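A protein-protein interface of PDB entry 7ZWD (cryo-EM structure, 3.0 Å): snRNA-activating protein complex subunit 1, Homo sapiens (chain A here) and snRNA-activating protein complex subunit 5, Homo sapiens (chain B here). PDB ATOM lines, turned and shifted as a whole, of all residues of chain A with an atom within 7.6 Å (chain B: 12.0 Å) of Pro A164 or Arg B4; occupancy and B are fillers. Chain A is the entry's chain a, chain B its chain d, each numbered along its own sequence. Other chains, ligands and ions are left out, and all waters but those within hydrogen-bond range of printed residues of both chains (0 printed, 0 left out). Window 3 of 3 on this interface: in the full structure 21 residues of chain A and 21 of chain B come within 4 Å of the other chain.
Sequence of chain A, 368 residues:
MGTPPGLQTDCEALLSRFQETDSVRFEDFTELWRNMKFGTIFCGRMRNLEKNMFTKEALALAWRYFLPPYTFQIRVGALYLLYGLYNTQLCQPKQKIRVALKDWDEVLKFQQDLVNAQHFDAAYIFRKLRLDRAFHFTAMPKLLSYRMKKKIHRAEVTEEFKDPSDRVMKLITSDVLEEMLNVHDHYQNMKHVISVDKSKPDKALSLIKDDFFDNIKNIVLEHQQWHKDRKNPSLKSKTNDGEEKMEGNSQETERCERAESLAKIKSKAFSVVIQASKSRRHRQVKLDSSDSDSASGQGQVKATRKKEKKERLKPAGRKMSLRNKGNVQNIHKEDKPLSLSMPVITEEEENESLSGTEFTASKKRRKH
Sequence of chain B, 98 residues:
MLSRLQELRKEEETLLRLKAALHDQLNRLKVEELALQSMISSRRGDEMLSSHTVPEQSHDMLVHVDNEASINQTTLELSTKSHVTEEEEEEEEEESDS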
ATOM      1  N   PRO A  68      -6.482  22.051 -19.813  1.00  0.00           N
ATOM      2  CA  PRO A  68      -5.352  22.705 -20.470  1.00  0.00           C
ATOM      3  C   PRO A  68      -5.786  23.363 -21.766  1.00  0.00           C
ATOM      4  O   PRO A  68      -6.839  23.021 -22.322  1.00  0.00           O
ATOM      5  CB  PRO A  68      -4.388  21.541 -20.730  1.00  0.00           C
ATOM      6  CG  PRO A  68      -4.643  20.625 -19.613  1.00  0.00           C
ATOM      7  CD  PRO A  68      -6.109  20.725 -19.294  1.00  0.00           C
ATOM      8  N   PRO A  69      -4.992  24.301 -22.301  1.00  0.00           N
ATOM      9  CA  PRO A  69      -3.653  24.693 -21.866  1.00  0.00           C
ATOM     10  C   PRO A  69      -3.650  25.881 -20.929  1.00  0.00           C
ATOM     11  O   PRO A  69      -2.878  26.803 -21.143  1.00  0.00           O
ATOM     12  CB  PRO A  69      -2.978  25.057 -23.179  1.00  0.00           C
ATOM     13  CG  PRO A  69      -4.089  25.674 -23.973  1.00  0.00           C
ATOM     14  CD  PRO A  69      -5.380  25.025 -23.523  1.00  0.00           C
ATOM     15  N   TYR A  70      -4.493  25.867 -19.910  1.00  0.00           N
ATOM     16  CA  TYR A  70      -4.630  27.007 -19.021  1.00  0.00           C
ATOM     17  C   TYR A  70      -3.783  26.821 -17.771  1.00  0.00           C
ATOM     18  O   TYR A  70      -3.363  25.711 -17.441  1.00  0.00           O
ATOM     19  CB  TYR A  70      -6.095  27.220 -18.648  1.00  0.00           C
ATOM     20  CG  TYR A  70      -6.905  27.764 -19.794  1.00  0.00           C
ATOM     21  CD1 TYR A  70      -7.321  29.080 -19.808  1.00  0.00           C
ATOM     22  CD2 TYR A  70      -7.222  26.968 -20.878  1.00  0.00           C
ATOM     23  CE1 TYR A  70      -8.048  29.581 -20.858  1.00  0.00           C
ATOM     24  CE2 TYR A  70      -7.945  27.461 -21.932  1.00  0.00           C
ATOM     25  CZ  TYR A  70      -8.355  28.768 -21.918  1.00  0.00           C
ATOM     26  OH  TYR A  70      -9.082  29.262 -22.972  1.00  0.00           O
ATOM     27  N   THR A  71      -3.528  27.931 -17.085  1.00  0.00           N
ATOM     28  CA  THR A  71      -2.723  27.899 -15.878  1.00  0.00           C
ATOM     29  C   THR A  71      -3.434  27.119 -14.784  1.00  0.00           C
ATOM     30  O   THR A  71      -4.654  26.941 -14.801  1.00  0.00           O
ATOM     31  CB  THR A  71      -2.439  29.309 -15.370  1.00  0.00           C
ATOM     32  OG1 THR A  71      -3.556  29.768 -14.600  1.00  0.00           O
ATOM     33  CG2 THR A  71      -2.211  30.258 -16.527  1.00  0.00           C
ATOM     34  N   PHE A  72      -2.648  26.658 -13.813  1.00  0.00           N
ATOM     35  CA  PHE A  72      -3.231  25.975 -12.667  1.00  0.00           C
ATOM     36  C   PHE A  72      -4.222  26.867 -11.942  1.00  0.00           C
ATOM     37  O   PHE A  72      -5.280  26.404 -11.503  1.00  0.00           O
ATOM     38  CB  PHE A  72      -2.137  25.523 -11.711  1.00  0.00           C
ATOM     39  CG  PHE A  72      -2.660  24.904 -10.457  1.00  0.00           C
ATOM     40  CD1 PHE A  72      -2.939  25.683  -9.349  1.00  0.00           C
ATOM     41  CD2 PHE A  72      -2.879  23.546 -10.385  1.00  0.00           C
ATOM     42  CE1 PHE A  72      -3.421  25.120  -8.199  1.00  0.00           C
ATOM     43  CE2 PHE A  72      -3.360  22.978  -9.233  1.00  0.00           C
ATOM     44  CZ  PHE A  72      -3.630  23.767  -8.140  1.00  0.00           C
ATOM     45  N   ILE A  74      -6.005  29.398 -13.186  1.00  0.00           N
ATOM     46  CA  ILE A  74      -7.203  29.467 -14.015  1.00  0.00           C
ATOM     47  C   ILE A  74      -7.976  28.161 -13.951  1.00  0.00           C
ATOM     48  O   ILE A  74      -9.209  28.158 -13.943  1.00  0.00           O
ATOM     49  CB  ILE A  74      -6.835  29.835 -15.464  1.00  0.00           C
ATOM     50  CG1 ILE A  74      -6.383  31.286 -15.537  1.00  0.00           C
ATOM     51  CG2 ILE A  74      -8.004  29.619 -16.387  1.00  0.00           C
ATOM     52  CD1 ILE A  74      -7.473  32.259 -15.140  1.00  0.00           C
ATOM     53  N   LYS A 162      -5.532  35.607 -23.273  1.00  0.00           N
ATOM     54  CA  LYS A 162      -5.878  34.627 -22.252  1.00  0.00           C
ATOM     55  C   LYS A 162      -4.696  34.387 -21.322  1.00  0.00           C
ATOM     56  O   LYS A 162      -3.787  35.211 -21.244  1.00  0.00           O
ATOM     57  CB  LYS A 162      -6.320  33.313 -22.895  1.00  0.00           C
ATOM     58  CG  LYS A 162      -7.609  33.405 -23.687  1.00  0.00           C
ATOM     59  CD  LYS A 162      -7.964  32.064 -24.293  1.00  0.00           C
ATOM     60  CE  LYS A 162      -8.822  32.227 -25.530  1.00  0.00           C
ATOM     61  NZ  LYS A 162      -8.473  31.236 -26.582  1.00  0.00           N
ATOM     62  N   ASP A 163      -4.713  33.258 -20.623  1.00  0.00           N
ATOM     63  CA  ASP A 163      -3.637  32.886 -19.706  1.00  0.00           C
ATOM     64  C   ASP A 163      -3.268  31.426 -19.926  1.00  0.00           C
ATOM     65  O   ASP A 163      -3.809  30.543 -19.229  1.00  0.00           O
ATOM     66  CB  ASP A 163      -4.051  33.134 -18.260  1.00  0.00           C
ATOM     67  CG  ASP A 163      -4.224  34.610 -17.952  1.00  0.00           C
ATOM     68  OD1 ASP A 163      -3.444  35.424 -18.485  1.00  0.00           O
ATOM     69  OD2 ASP A 163      -5.139  34.958 -17.176  1.00  0.00           O
ATOM     70  N   PRO A 164      -2.388  31.125 -20.873  1.00  0.00           N
ATOM     71  CA  PRO A 164      -2.000  29.739 -21.136  1.00  0.00           C
ATOM     72  C   PRO A 164      -0.725  29.325 -20.410  1.00  0.00           C
ATOM     73  O   PRO A 164      -0.084  30.110 -19.711  1.00  0.00           O
ATOM     74  CB  PRO A 164      -1.786  29.737 -22.654  1.00  0.00           C
ATOM     75  CG  PRO A 164      -1.265  31.110 -22.935  1.00  0.00           C
ATOM     76  CD  PRO A 164      -1.841  32.043 -21.885  1.00  0.00           C
ATOM     77  N   SER A 165      -0.375  28.051 -20.591  1.00  0.00           N
ATOM     78  CA  SER A 165       0.853  27.464 -20.063  1.00  0.00           C
ATOM     79  C   SER A 165       1.787  27.146 -21.223  1.00  0.00           C
ATOM     80  O   SER A 165       1.343  26.649 -22.263  1.00  0.00           O
ATOM     81  CB  SER A 165       0.558  26.203 -19.252  1.00  0.00           C
ATOM     82  OG  SER A 165       1.635  25.888 -18.386  1.00  0.00           O
ATOM     83  N   ASP A 166       3.075  27.428 -21.041  1.00  0.00           N
ATOM     84  CA  ASP A 166       4.077  27.308 -22.089  1.00  0.00           C
ATOM     85  C   ASP A 166       4.872  26.015 -21.946  1.00  0.00           C
ATOM     86  O   ASP A 166       4.967  25.431 -20.864  1.00  0.00           O
ATOM     87  CB  ASP A 166       5.038  28.503 -22.061  1.00  0.00           C
ATOM     88  CG  ASP A 166       4.314  29.833 -22.087  1.00  0.00           C
ATOM     89  OD1 ASP A 166       3.067  29.837 -22.140  1.00  0.00           O
ATOM     90  OD2 ASP A 166       4.996  30.878 -22.050  1.00  0.00           O
ATOM     91  N   ARG A 167       5.453  25.576 -23.065  1.00  0.00           N
ATOM     92  CA  ARG A 167       6.353  24.427 -23.034  1.00  0.00           C
ATOM     93  C   ARG A 167       7.692  24.778 -22.401  1.00  0.00           C
ATOM     94  O   ARG A 167       8.407  23.884 -21.934  1.00  0.00           O
ATOM     95  CB  ARG A 167       6.590  23.888 -24.447  1.00  0.00           C
ATOM     96  CG  ARG A 167       5.528  22.937 -24.981  1.00  0.00           C
ATOM     97  CD  ARG A 167       5.959  22.390 -26.339  1.00  0.00           C
ATOM     98  NE  ARG A 167       5.088  21.331 -26.837  1.00  0.00           N
ATOM     99  CZ  ARG A 167       4.069  21.526 -27.669  1.00  0.00           C
ATOM    100  NH1 ARG A 167       3.787  22.747 -28.103  1.00  0.00           N
ATOM    101  NH2 ARG A 167       3.334  20.499 -28.073  1.00  0.00           N
ATOM    102  N   MET A 169       8.478  26.487 -19.696  1.00  0.00           N
ATOM    103  CA  MET A 169       8.554  26.244 -18.260  1.00  0.00           C
ATOM    104  C   MET A 169       8.615  24.755 -17.950  1.00  0.00           C
ATOM    105  O   MET A 169       9.255  24.353 -16.972  1.00  0.00           O
ATOM    106  CB  MET A 169       7.374  26.897 -17.540  1.00  0.00           C
ATOM    107  CG  MET A 169       6.012  26.633 -18.161  1.00  0.00           C
ATOM    108  SD  MET A 169       4.688  27.477 -17.270  1.00  0.00           S
ATOM    109  CE  MET A 169       4.307  28.827 -18.384  1.00  0.00           C
ATOM    110  N   HIS A 227       7.461  37.891 -25.958  1.00  0.00           N
ATOM    111  CA  HIS A 227       6.130  37.665 -25.410  1.00  0.00           C
ATOM    112  C   HIS A 227       5.525  38.965 -24.888  1.00  0.00           C
ATOM    113  O   HIS A 227       4.340  39.244 -25.119  1.00  0.00           O
ATOM    114  CB  HIS A 227       6.193  36.606 -24.308  1.00  0.00           C
ATOM    115  CG  HIS A 227       4.921  35.836 -24.135  1.00  0.00           C
ATOM    116  ND1 HIS A 227       4.699  34.993 -23.068  1.00  0.00           N
ATOM    117  CD2 HIS A 227       3.805  35.772 -24.901  1.00  0.00           C
ATOM    118  CE1 HIS A 227       3.501  34.447 -23.180  1.00  0.00           C
ATOM    119  NE2 HIS A 227       2.938  34.903 -24.284  1.00  0.00           N
ATOM    120  N   ARG A 230       4.687  41.271 -27.590  1.00  0.00           N
ATOM    121  CA  ARG A 230       3.471  40.795 -28.239  1.00  0.00           C
ATOM    122  C   ARG A 230       2.235  41.229 -27.463  1.00  0.00           C
ATOM    123  O   ARG A 230       1.298  41.794 -28.038  1.00  0.00           O
ATOM    124  CB  ARG A 230       3.499  39.272 -28.389  1.00  0.00           C
ATOM    125  CG  ARG A 230       2.187  38.683 -28.906  1.00  0.00           C
ATOM    126  CD  ARG A 230       2.325  37.203 -29.235  1.00  0.00           C
ATOM    127  NE  ARG A 230       1.145  36.662 -29.909  1.00  0.00           N
ATOM    128  CZ  ARG A 230       1.101  35.469 -30.498  1.00  0.00           C
ATOM    129  NH1 ARG A 230       2.169  34.685 -30.499  1.00  0.00           N
ATOM    130  NH2 ARG A 230      -0.011  35.054 -31.086  1.00  0.00           N
ATOM    131  N   MET B   1      -7.548  31.476 -35.713  1.00  0.00           N
ATOM    132  CA  MET B   1      -6.712  30.563 -34.943  1.00  0.00           C
ATOM    133  C   MET B   1      -5.243  30.910 -35.112  1.00  0.00           C
ATOM    134  O   MET B   1      -4.369  30.268 -34.525  1.00  0.00           O
ATOM    135  CB  MET B   1      -6.956  29.117 -35.370  1.00  0.00           C
ATOM    136  CG  MET B   1      -6.582  28.827 -36.808  1.00  0.00           C
ATOM    137  SD  MET B   1      -7.323  27.292 -37.383  1.00  0.00           S
ATOM    138  CE  MET B   1      -7.120  26.258 -35.936  1.00  0.00           C
ATOM    139  N   LEU B   2      -4.974  31.936 -35.923  1.00  0.00           N
ATOM    140  CA  LEU B   2      -3.591  32.316 -36.179  1.00  0.00           C
ATOM    141  C   LEU B   2      -2.915  32.850 -34.926  1.00  0.00           C
ATOM    142  O   LEU B   2      -1.691  32.791 -34.821  1.00  0.00           O
ATOM    143  CB  LEU B   2      -3.511  33.355 -37.295  1.00  0.00           C
ATOM    144  CG  LEU B   2      -3.221  32.879 -38.719  1.00  0.00           C
ATOM    145  CD1 LEU B   2      -3.186  34.071 -39.660  1.00  0.00           C
ATOM    146  CD2 LEU B   2      -1.937  32.077 -38.801  1.00  0.00           C
ATOM    147  N   SER B   3      -3.680  33.396 -33.978  1.00  0.00           N
ATOM    148  CA  SER B   3      -3.087  33.788 -32.703  1.00  0.00           C
ATOM    149  C   SER B   3      -2.467  32.585 -32.007  1.00  0.00           C
ATOM    150  O   SER B   3      -1.278  32.594 -31.655  1.00  0.00           O
ATOM    151  CB  SER B   3      -4.144  34.434 -31.807  1.00  0.00           C
ATOM    152  OG  SER B   3      -4.368  35.790 -32.151  1.00  0.00           O
ATOM    153  N   ARG B   4      -3.261  31.531 -31.815  1.00  0.00           N
ATOM    154  CA  ARG B   4      -2.736  30.300 -31.245  1.00  0.00           C
ATOM    155  C   ARG B   4      -1.658  29.701 -32.136  1.00  0.00           C
ATOM    156  O   ARG B   4      -0.656  29.182 -31.637  1.00  0.00           O
ATOM    157  CB  ARG B   4      -3.868  29.301 -31.021  1.00  0.00           C
ATOM    158  CG  ARG B   4      -3.454  28.077 -30.228  1.00  0.00           C
ATOM    159  CD  ARG B   4      -2.944  28.467 -28.851  1.00  0.00           C
ATOM    160  NE  ARG B   4      -1.508  28.245 -28.722  1.00  0.00           N
ATOM    161  CZ  ARG B   4      -0.813  28.500 -27.620  1.00  0.00           C
ATOM    162  NH1 ARG B   4      -1.424  28.987 -26.550  1.00  0.00           N
ATOM    163  NH2 ARG B   4       0.492  28.272 -27.588  1.00  0.00           N
ATOM    164  N   LEU B   5      -1.843  29.766 -33.457  1.00  0.00           N
ATOM    165  CA  LEU B   5      -0.860  29.189 -34.367  1.00  0.00           C
ATOM    166  C   LEU B   5       0.498  29.867 -34.209  1.00  0.00           C
ATOM    167  O   LEU B   5       1.541  29.200 -34.203  1.00  0.00           O
ATOM    168  CB  LEU B   5      -1.370  29.292 -35.807  1.00  0.00           C
ATOM    169  CG  LEU B   5      -0.661  28.514 -36.919  1.00  0.00           C
ATOM    170  CD1 LEU B   5      -1.649  28.147 -38.020  1.00  0.00           C
ATOM    171  CD2 LEU B   5       0.503  29.301 -37.500  1.00  0.00           C
ATOM    172  N   GLN B   6       0.503  31.192 -34.045  1.00  0.00           N
ATOM    173  CA  GLN B   6       1.764  31.907 -33.894  1.00  0.00           C
ATOM    174  C   GLN B   6       2.356  31.700 -32.510  1.00  0.00           C
ATOM    175  O   GLN B   6       3.580  31.631 -32.361  1.00  0.00           O
ATOM    176  CB  GLN B   6       1.578  33.396 -34.181  1.00  0.00           C
ATOM    177  CG  GLN B   6       1.047  33.706 -35.572  1.00  0.00           C
ATOM    178  CD  GLN B   6       1.745  32.933 -36.677  1.00  0.00           C
ATOM    179  OE1 GLN B   6       2.938  32.649 -36.605  1.00  0.00           O
ATOM    180  NE2 GLN B   6       0.995  32.594 -37.712  1.00  0.00           N
ATOM    181  N   GLU B   7       1.510  31.588 -31.486  1.00  0.00           N
ATOM    182  CA  GLU B   7       2.025  31.219 -30.172  1.00  0.00           C
ATOM    183  C   GLU B   7       2.734  29.870 -30.235  1.00  0.00           C
ATOM    184  O   GLU B   7       3.851  29.711 -29.721  1.00  0.00           O
ATOM    185  CB  GLU B   7       0.890  31.201 -29.149  1.00  0.00           C
ATOM    186  CG  GLU B   7       0.652  32.546 -28.476  1.00  0.00           C
ATOM    187  CD  GLU B   7      -0.407  32.487 -27.395  1.00  0.00           C
ATOM    188  OE1 GLU B   7      -0.665  33.528 -26.756  1.00  0.00           O
ATOM    189  OE2 GLU B   7      -0.988  31.404 -27.185  1.00  0.00           O
ATOM    190  N   LEU B   8       2.109  28.894 -30.899  1.00  0.00           N
ATOM    191  CA  LEU B   8       2.707  27.567 -31.005  1.00  0.00           C
ATOM    192  C   LEU B   8       3.991  27.591 -31.826  1.00  0.00           C
ATOM    193  O   LEU B   8       4.968  26.927 -31.467  1.00  0.00           O
ATOM    194  CB  LEU B   8       1.710  26.572 -31.604  1.00  0.00           C
ATOM    195  CG  LEU B   8       0.333  26.408 -30.958  1.00  0.00           C
ATOM    196  CD1 LEU B   8      -0.626  25.707 -31.911  1.00  0.00           C
ATOM    197  CD2 LEU B   8       0.433  25.653 -29.641  1.00  0.00           C
ATOM    198  N   ARG B   9       4.023  28.355 -32.924  1.00  0.00           N
ATOM    199  CA  ARG B   9       5.244  28.390 -33.727  1.00  0.00           C
ATOM    200  C   ARG B   9       6.371  29.090 -32.978  1.00  0.00           C
ATOM    201  O   ARG B   9       7.541  28.728 -33.134  1.00  0.00           O
ATOM    202  CB  ARG B   9       5.000  29.065 -35.081  1.00  0.00           C
ATOM    203  CG  ARG B   9       4.641  30.527 -34.998  1.00  0.00           C
ATOM    204  CD  ARG B   9       5.882  31.430 -35.001  1.00  0.00           C
ATOM    205  NE  ARG B   9       5.574  32.820 -34.683  1.00  0.00           N
ATOM    206  CZ  ARG B   9       6.488  33.720 -34.334  1.00  0.00           C
ATOM    207  NH1 ARG B   9       7.764  33.363 -34.255  1.00  0.00           N
ATOM    208  NH2 ARG B   9       6.125  34.966 -34.055  1.00  0.00           N
ATOM    209  N   LYS B  10       6.049  30.123 -32.193  1.00  0.00           N
ATOM    210  CA  LYS B  10       7.083  30.806 -31.425  1.00  0.00           C
ATOM    211  C   LYS B  10       7.652  29.881 -30.364  1.00  0.00           C
ATOM    212  O   LYS B  10       8.873  29.824 -30.159  1.00  0.00           O
ATOM    213  CB  LYS B  10       6.518  32.070 -30.784  1.00  0.00           C
ATOM    214  CG  LYS B  10       7.474  32.730 -29.804  1.00  0.00           C
ATOM    215  CD  LYS B  10       8.762  33.170 -30.482  1.00  0.00           C
ATOM    216  CE  LYS B  10       9.730  33.782 -29.485  1.00  0.00           C
ATOM    217  NZ  LYS B  10      10.995  34.208 -30.138  1.00  0.00           N
ATOM    218  N   GLU B  11       6.775  29.147 -29.676  1.00  0.00           N
ATOM    219  CA  GLU B  11       7.247  28.076 -28.814  1.00  0.00           C
ATOM    220  C   GLU B  11       8.117  27.092 -29.581  1.00  0.00           C
ATOM    221  O   GLU B  11       9.120  26.608 -29.046  1.00  0.00           O
ATOM    222  CB  GLU B  11       6.063  27.351 -28.179  1.00  0.00           C
ATOM    223  CG  GLU B  11       5.508  28.043 -26.956  1.00  0.00           C
ATOM    224  CD  GLU B  11       5.063  27.061 -25.898  1.00  0.00           C
ATOM    225  OE1 GLU B  11       4.120  26.286 -26.159  1.00  0.00           O
ATOM    226  OE2 GLU B  11       5.679  27.047 -24.815  1.00  0.00           O
ATOM    227  N   GLU B  12       7.763  26.808 -30.835  1.00  0.00           N
ATOM    228  CA  GLU B  12       8.523  25.852 -31.631  1.00  0.00           C
ATOM    229  C   GLU B  12       9.933  26.358 -31.900  1.00  0.00           C
ATOM    230  O   GLU B  12      10.907  25.611 -31.777  1.00  0.00           O
ATOM    231  CB  GLU B  12       7.785  25.571 -32.940  1.00  0.00           C
ATOM    232  CG  GLU B  12       8.411  24.502 -33.808  1.00  0.00           C
ATOM    233  CD  GLU B  12       7.936  24.585 -35.240  1.00  0.00           C
ATOM    234  OE1 GLU B  12       8.677  25.125 -36.084  1.00  0.00           O
ATOM    235  OE2 GLU B  12       6.816  24.111 -35.523  1.00  0.00           O
ATOM    236  N   GLU B  13      10.060  27.629 -32.277  1.00  0.00           N
ATOM    237  CA  GLU B  13      11.386  28.190 -32.529  1.00  0.00           C
ATOM    238  C   GLU B  13      12.203  28.262 -31.247  1.00  0.00           C
ATOM    239  O   GLU B  13      13.414  28.004 -31.256  1.00  0.00           O
ATOM    240  CB  GLU B  13      11.277  29.572 -33.177  1.00  0.00           C
ATOM    241  CG  GLU B  13      10.187  29.716 -34.235  1.00  0.00           C
ATOM    242  CD  GLU B  13      10.165  28.592 -35.266  1.00  0.00           C
ATOM    243  OE1 GLU B  13       9.083  28.345 -35.838  1.00  0.00           O
ATOM    244  OE2 GLU B  13      11.222  27.984 -35.539  1.00  0.00           O
ATOM    245  N   THR B  14      11.557  28.592 -30.125  1.00  0.00           N
ATOM    246  CA  THR B  14      12.265  28.595 -28.849  1.00  0.00           C
ATOM    247  C   THR B  14      12.791  27.206 -28.508  1.00  0.00           C
ATOM    248  O   THR B  14      13.960  27.049 -28.127  1.00  0.00           O
ATOM    249  CB  THR B  14      11.345  29.108 -27.741  1.00  0.00           C
ATOM    250  OG1 THR B  14      10.606  30.239 -28.218  1.00  0.00           O
ATOM    251  CG2 THR B  14      12.155  29.517 -26.516  1.00  0.00           C
ATOM    252  N   LEU B  15      11.948  26.181 -28.648  1.00  0.00           N
ATOM    253  CA  LEU B  15      12.382  24.835 -28.300  1.00  0.00           C
ATOM    254  C   LEU B  15      13.407  24.300 -29.294  1.00  0.00           C
ATOM    255  O   LEU B  15      14.288  23.532 -28.903  1.00  0.00           O
ATOM    256  CB  LEU B  15      11.175  23.896 -28.168  1.00  0.00           C
ATOM    257  CG  LEU B  15      10.139  23.684 -29.274  1.00  0.00           C
ATOM    258  CD1 LEU B  15      10.508  22.537 -30.187  1.00  0.00           C
ATOM    259  CD2 LEU B  15       8.764  23.449 -28.664  1.00  0.00           C
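OE1 of Glu B11 sits close to N of Arg A167, 3.4 Å away. The guanidinium group of Arg A230 is in hydrogen-bond range of the backbone carbonyl oxygen of Ser B3 (2.8 Å). The backbone NH (N) of Glu B7 sits close to the guanidinium group (NH1) of Arg A230 (3.3 Å).
OE2 of Glu B7 lies within salt-bridge range of NH1 of Arg B4 (2.5 Å). The side-chain amide oxygen of Gln B6 sits close to the guanidinium group of Arg B9.
Among the printed residues, merely in contact across the chains: Asp A166 with Glu B11, Arg A230 with Gln B6, Arg A167 with Leu B15 and Pro A164 with Arg B4.
Printed residues of chain B within 4 Å of Pro A164: Arg B4 (3.98 Å). Of the printed residues of chain A, Arg B4 touches Pro A164. No residue of chain B comes within 4 Å of Tyr A70. No residue of chain B comes within 4 Å of Thr A71. No residue of chain B comes within 4 Å of Lys A162. No residue of chain B comes within 4 Å of Asp A163. No residue of chain B comes within 4 Å of Ser A165. Of chain B, only Glu B11 comes within 4 Å of Asp A166. Printed residues of chain B within 4 Å of Arg A230: Ser B3 (2.8 Å), Gln B6 (3.6 Å) and Glu B7 (3.3 Å). Printed residues of chain A within 4 Å of Glu B11: Asp A166 (3.2 Å) and Arg A167 (2.3 Å). His A227 touches none of the printed residues of chain B.
Hydrophobic or aromatic side chains of chain A that line the printed part of chain B: Pro A164. Hydrophobic or aromatic side chains of chain B that line the printed part of chain A: Leu B15. Among the printed residues, no Asp or Glu carboxylate lies within 4 Å of a Lys or Arg side-chain nitrogen of the other chain.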
